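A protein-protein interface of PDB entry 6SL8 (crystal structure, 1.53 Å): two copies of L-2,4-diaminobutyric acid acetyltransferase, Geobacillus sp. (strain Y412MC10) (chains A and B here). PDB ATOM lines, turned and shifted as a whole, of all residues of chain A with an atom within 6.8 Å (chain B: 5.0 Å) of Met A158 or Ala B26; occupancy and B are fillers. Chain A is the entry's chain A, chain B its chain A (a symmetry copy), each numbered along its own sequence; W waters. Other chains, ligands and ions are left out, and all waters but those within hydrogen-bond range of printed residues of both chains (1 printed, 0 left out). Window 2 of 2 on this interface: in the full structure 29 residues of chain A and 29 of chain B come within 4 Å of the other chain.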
ATOM      1  N   GLY A 153       2.711  26.623  -2.894  1.00  0.00           N
ATOM      2  CA  GLY A 153       2.863  26.865  -1.449  1.00  0.00           C
ATOM      3  C   GLY A 153       4.370  26.998  -1.221  1.00  0.00           C
ATOM      4  O   GLY A 153       4.945  28.056  -1.522  1.00  0.00           O
ATOM      5  N   TYR A 154       5.004  26.018  -0.651  1.00  0.00           N
ATOM      6  CA  TYR A 154       6.476  26.129  -0.447  1.00  0.00           C
ATOM      7  C   TYR A 154       7.100  25.122  -1.446  1.00  0.00           C
ATOM      8  O   TYR A 154       6.995  23.905  -1.304  1.00  0.00           O
ATOM      9  CB  TYR A 154       6.861  25.729   0.999  1.00  0.00           C
ATOM     10  CG  TYR A 154       6.137  26.468   2.125  1.00  0.00           C
ATOM     11  CD1 TYR A 154       5.933  27.783   2.079  1.00  0.00           C
ATOM     12  CD2 TYR A 154       5.687  25.769   3.174  1.00  0.00           C
ATOM     13  CE1 TYR A 154       5.188  28.452   3.109  1.00  0.00           C
ATOM     14  CE2 TYR A 154       5.011  26.392   4.206  1.00  0.00           C
ATOM     15  CZ  TYR A 154       4.784  27.686   4.156  1.00  0.00           C
ATOM     16  OH  TYR A 154       4.041  28.376   5.185  1.00  0.00           O
ATOM     17  N   GLY A 155       7.832  25.689  -2.396  1.00  0.00           N
ATOM     18  CA  GLY A 155       8.408  24.824  -3.373  1.00  0.00           C
ATOM     19  C   GLY A 155       9.646  24.083  -2.824  1.00  0.00           C
ATOM     20  O   GLY A 155      10.306  24.556  -1.880  1.00  0.00           O
ATOM     21  N   ALA A 156      10.008  22.990  -3.487  1.00  0.00           N
ATOM     22  CA  ALA A 156      11.155  22.164  -3.123  1.00  0.00           C
ATOM     23  C   ALA A 156      12.388  23.038  -2.984  1.00  0.00           C
ATOM     24  O   ALA A 156      13.228  22.767  -2.100  1.00  0.00           O
ATOM     25  CB  ALA A 156      11.398  21.061  -4.150  1.00  0.00           C
ATOM     26  N   GLU A 157      12.526  24.051  -3.828  1.00  0.00           N
ATOM     27  CA  GLU A 157      13.660  24.950  -3.862  1.00  0.00           C
ATOM     28  C   GLU A 157      13.875  25.832  -2.641  1.00  0.00           C
ATOM     29  O   GLU A 157      14.973  26.338  -2.445  1.00  0.00           O
ATOM     30  CB  GLU A 157      13.715  25.870  -5.096  1.00  0.00           C
ATOM     31  CG  GLU A 157      12.592  26.865  -5.294  1.00  0.00           C
ATOM     32  CD  GLU A 157      11.282  26.296  -5.787  1.00  0.00           C
ATOM     33  OE1 GLU A 157      11.036  25.102  -5.886  1.00  0.00           O
ATOM     34  OE2 GLU A 157      10.405  27.119  -6.095  1.00  0.00           O
ATOM     35  N   MET A 158      12.856  25.883  -1.785  1.00  0.00           N
ATOM     36  CA  MET A 158      12.977  26.677  -0.533  1.00  0.00           C
ATOM     37  C   MET A 158      13.651  25.883   0.556  1.00  0.00           C
ATOM     38  O   MET A 158      13.952  26.463   1.606  1.00  0.00           O
ATOM     39  CB  MET A 158      11.524  27.022  -0.069  1.00  0.00           C
ATOM     40  CG  MET A 158      10.837  27.994  -0.996  1.00  0.00           C
ATOM     41  SD  MET A 158       9.216  28.558  -0.303  1.00  0.00           S
ATOM     42  CE  MET A 158       9.538  28.981   1.490  1.00  0.00           C
ATOM     43  N   PHE A 159      13.771  24.582   0.422  1.00  0.00           N
ATOM     44  CA  PHE A 159      14.282  23.661   1.439  1.00  0.00           C
ATOM     45  C   PHE A 159      15.814  23.659   1.464  1.00  0.00           C
ATOM     46  O   PHE A 159      16.430  24.113   0.497  1.00  0.00           O
ATOM     47  CB  PHE A 159      13.673  22.303   1.371  1.00  0.00           C
ATOM     48  CG  PHE A 159      12.172  22.322   1.725  1.00  0.00           C
ATOM     49  CD1 PHE A 159      11.204  22.724   0.829  1.00  0.00           C
ATOM     50  CD2 PHE A 159      11.774  21.982   3.008  1.00  0.00           C
ATOM     51  CE1 PHE A 159       9.854  22.843   1.206  1.00  0.00           C
ATOM     52  CE2 PHE A 159      10.412  22.028   3.394  1.00  0.00           C
ATOM     53  CZ  PHE A 159       9.459  22.496   2.522  1.00  0.00           C
ATOM     54  N   PRO A 160      16.412  23.153   2.556  1.00  0.00           N
ATOM     55  CA  PRO A 160      17.861  23.281   2.718  1.00  0.00           C
ATOM     56  C   PRO A 160      18.644  22.488   1.705  1.00  0.00           C
ATOM     57  O   PRO A 160      18.224  21.384   1.305  1.00  0.00           O
ATOM     58  CB  PRO A 160      18.103  22.715   4.120  1.00  0.00           C
ATOM     59  CG  PRO A 160      16.819  23.008   4.910  1.00  0.00           C
ATOM     60  CD  PRO A 160      15.794  22.689   3.842  1.00  0.00           C
ATOM     61  N   ASP A 161      19.794  23.074   1.379  1.00  0.00           N
ATOM     62  CA  ASP A 161      20.836  22.304   0.679  1.00  0.00           C
ATOM     63  C   ASP A 161      21.197  21.135   1.579  1.00  0.00           C
ATOM     64  O   ASP A 161      21.376  21.273   2.853  1.00  0.00           O
ATOM     65  CB  ASP A 161      22.121  23.110   0.487  1.00  0.00           C
ATOM     66  CG  ASP A 161      21.968  24.292  -0.468  1.00  0.00           C
ATOM     67  OD1 ASP A 161      20.992  24.391  -1.216  1.00  0.00           O
ATOM     68  OD2 ASP A 161      22.851  25.155  -0.444  1.00  0.00           O
ATOM     69  N   PRO B  24      10.455  37.789  10.372  1.00  0.00           N
ATOM     70  CA  PRO B  24      10.778  36.798   9.356  1.00  0.00           C
ATOM     71  C   PRO B  24       9.664  36.679   8.342  1.00  0.00           C
ATOM     72  O   PRO B  24       8.545  37.118   8.605  1.00  0.00           O
ATOM     73  CB  PRO B  24      10.915  35.467  10.137  1.00  0.00           C
ATOM     74  CG  PRO B  24       9.995  35.724  11.296  1.00  0.00           C
ATOM     75  CD  PRO B  24      10.189  37.151  11.689  1.00  0.00           C
ATOM     76  N   GLU B  25       9.989  36.008   7.252  1.00  0.00           N
ATOM     77  CA  GLU B  25       9.023  35.622   6.234  1.00  0.00           C
ATOM     78  C   GLU B  25       9.191  34.154   6.004  1.00  0.00           C
ATOM     79  O   GLU B  25      10.197  33.557   6.360  1.00  0.00           O
ATOM     80  CB  GLU B  25       9.275  36.444   4.930  1.00  0.00           C
ATOM     81  CG  GLU B  25       9.148  37.970   5.158  1.00  0.00           C
ATOM     82  CD  GLU B  25       7.695  38.467   5.487  1.00  0.00           C
ATOM     83  OE1 GLU B  25       7.568  39.578   6.086  1.00  0.00           O
ATOM     84  OE2 GLU B  25       6.677  37.765   5.167  1.00  0.00           O
ATOM     85  N   ALA B  26       8.244  33.512   5.321  1.00  0.00           N
ATOM     86  CA  ALA B  26       8.342  32.079   5.021  1.00  0.00           C
ATOM     87  C   ALA B  26       9.674  31.752   4.322  1.00  0.00           C
ATOM     88  O   ALA B  26      10.277  30.746   4.580  1.00  0.00           O
ATOM     89  CB  ALA B  26       7.179  31.612   4.170  1.00  0.00           C
ATOM     90  N   ARG B  27      10.117  32.660   3.415  1.00  0.00           N
ATOM     91  CA  ARG B  27      11.335  32.412   2.641  1.00  0.00           C
ATOM     92  C   ARG B  27      12.590  32.323   3.503  1.00  0.00           C
ATOM     93  O   ARG B  27      13.642  31.803   3.042  1.00  0.00           O
ATOM     94  CB  ARG B  27      11.578  33.472   1.502  1.00  0.00           C
ATOM     95  CG  ARG B  27      11.694  34.887   1.957  1.00  0.00           C
ATOM     96  CD  ARG B  27      12.289  35.982   1.005  1.00  0.00           C
ATOM     97  NE  ARG B  27      13.677  36.397   1.403  1.00  0.00           N
ATOM     98  CZ  ARG B  27      14.081  37.020   2.550  1.00  0.00           C
ATOM     99  NH1 ARG B  27      15.379  37.294   2.718  1.00  0.00           N
ATOM    100  NH2 ARG B  27      13.241  37.373   3.552  1.00  0.00           N
ATOM    101  N   ASP B  28      12.537  32.866   4.737  1.00  0.00           N
ATOM    102  CA  ASP B  28      13.667  32.784   5.677  1.00  0.00           C
ATOM    103  C   ASP B  28      13.781  31.430   6.362  1.00  0.00           C
ATOM    104  O   ASP B  28      14.757  31.163   7.089  1.00  0.00           O
ATOM    105  CB  ASP B  28      13.475  33.848   6.744  1.00  0.00           C
ATOM    106  CG  ASP B  28      13.537  35.215   6.219  1.00  0.00           C
ATOM    107  OD1 ASP B  28      14.504  35.521   5.430  1.00  0.00           O
ATOM    108  OD2 ASP B  28      12.639  35.986   6.479  1.00  0.00           O
ATOM    109  N   GLY B  29      12.806  30.520   6.147  1.00  0.00           N
ATOM    110  CA  GLY B  29      12.799  29.262   6.835  1.00  0.00           C
ATOM    111  C   GLY B  29      14.077  28.470   6.888  1.00  0.00           C
ATOM    112  O   GLY B  29      14.536  27.996   7.906  1.00  0.00           O
ATOM    113  N   THR B  30      14.643  28.241   5.709  1.00  0.00           N
ATOM    114  CA  THR B  30      15.884  27.491   5.618  1.00  0.00           C
ATOM    115  C   THR B  30      17.124  28.161   6.320  1.00  0.00           C
ATOM    116  O   THR B  30      17.816  27.451   7.064  1.00  0.00           O
ATOM    117  CB  THR B  30      16.179  27.220   4.113  1.00  0.00           C
ATOM    118  OG1 THR B  30      15.384  26.068   3.767  1.00  0.00           O
ATOM    119  CG2 THR B  30      17.701  26.870   3.889  1.00  0.00           C
ATOM    120  N   MET B  51       9.533  27.733   8.212  1.00  0.00           N
ATOM    121  CA  MET B  51       8.731  28.376   7.160  1.00  0.00           C
ATOM    122  C   MET B  51       7.388  28.805   7.705  1.00  0.00           C
ATOM    123  O   MET B  51       6.979  29.919   7.456  1.00  0.00           O
ATOM    124  CB  MET B  51       8.614  27.482   5.948  1.00  0.00           C
ATOM    125  CG  MET B  51       9.903  27.160   5.332  1.00  0.00           C
ATOM    126  SD  MET B  51       9.616  25.929   4.006  1.00  0.00           S
ATOM    127  CE  MET B  51      11.324  25.472   3.694  1.00  0.00           C
ATOM    128  N   GLY B  54       7.615  31.852   9.980  1.00  0.00           N
ATOM    129  CA  GLY B  54       7.690  33.112   9.242  1.00  0.00           C
ATOM    130  C   GLY B  54       6.437  33.467   8.448  1.00  0.00           C
ATOM    131  O   GLY B  54       6.203  34.635   8.220  1.00  0.00           O
ATOM    132  N   ASP B  55       5.629  32.500   8.031  1.00  0.00           N
ATOM    133  CA  ASP B  55       4.419  32.758   7.238  1.00  0.00           C
ATOM    134  C   ASP B  55       3.274  33.181   8.170  1.00  0.00           C
ATOM    135  O   ASP B  55       2.573  34.146   7.894  1.00  0.00           O
ATOM    136  CB  ASP B  55       4.059  31.487   6.540  1.00  0.00           C
ATOM    137  CG  ASP B  55       3.274  31.678   5.247  1.00  0.00           C
ATOM    138  OD1 ASP B  55       2.980  32.819   4.920  1.00  0.00           O
ATOM    139  OD2 ASP B  55       3.122  30.685   4.514  1.00  0.00           O
HETATM  140  O   HOH W   1      13.196  28.804   3.159  1.00  0.00           O
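Printed residues of chain B within 4 Å of Met A158: Ala B26, Thr B30 and Met B51. Of the printed residues of chain B, Phe A159 touches Thr B30 (3.4 Å) and Met B51 (3.6 Å). Of the printed residues of chain A, Asp B55 touches Tyr A154 (2.6 Å). Of the printed residues of chain B, Tyr A154 touches Ala B26, Met B51 and Asp B55. Of the printed residues of chain B, Pro A160 touches Thr B30 (3.3 Å). Gly B54 touches none of the printed residues of chain A. The nearest printed residue of chain B that does not touch Phe A159 is Gly B29 (7.3 Å).
Among the printed residues, pairs that only touch across the chains: Phe A159 with Thr B30, Met A158 with Met B51, Phe A159 with Met B51, Met A158 with Ala B26, Tyr A154 with Ala B26 and Tyr A154 with Met B51.
No position is printed for both chains. Of the 9 pairs that touch across the chains among the printed residues, none has its exchanged pair printed and touching as well.
Water W1 lies within hydrogen-bond range of the backbone carbonyl oxygen of Met A158 (2.9 Å), the backbone NH of Thr B30 (3.0 Å), the backbone carbonyl oxygen of Arg B27 (3.0 Å) and the backbone NH of Gly B29 (3.5 Å).
The side-chain hydroxyl of Thr B30 lies within hydrogen-bond range of the backbone carbonyl oxygen of Met A158 (2.6 Å). The backbone nitrogen of Pro A160 sits close to the side-chain hydroxyl of Thr B30, at 3.3 Å. The side-chain hydroxyl of Tyr A154 lies within hydrogen-bond range of the side-chain carboxylate of Asp B55, at 2.6 Å.
Hydrophobic or aromatic side chains of chain B within 4 Å of the printed part of chain A: Ala B26 and Met B51. Along chain A the printed residues that touch a printed residue of chain B span positions 154 to 160. Among the printed residues, 9 pairs touch across the chains. Among the printed residues, no Asp or Glu carboxylate lies within 4 Å of a Lys or Arg side-chain nitrogen of the other chain.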
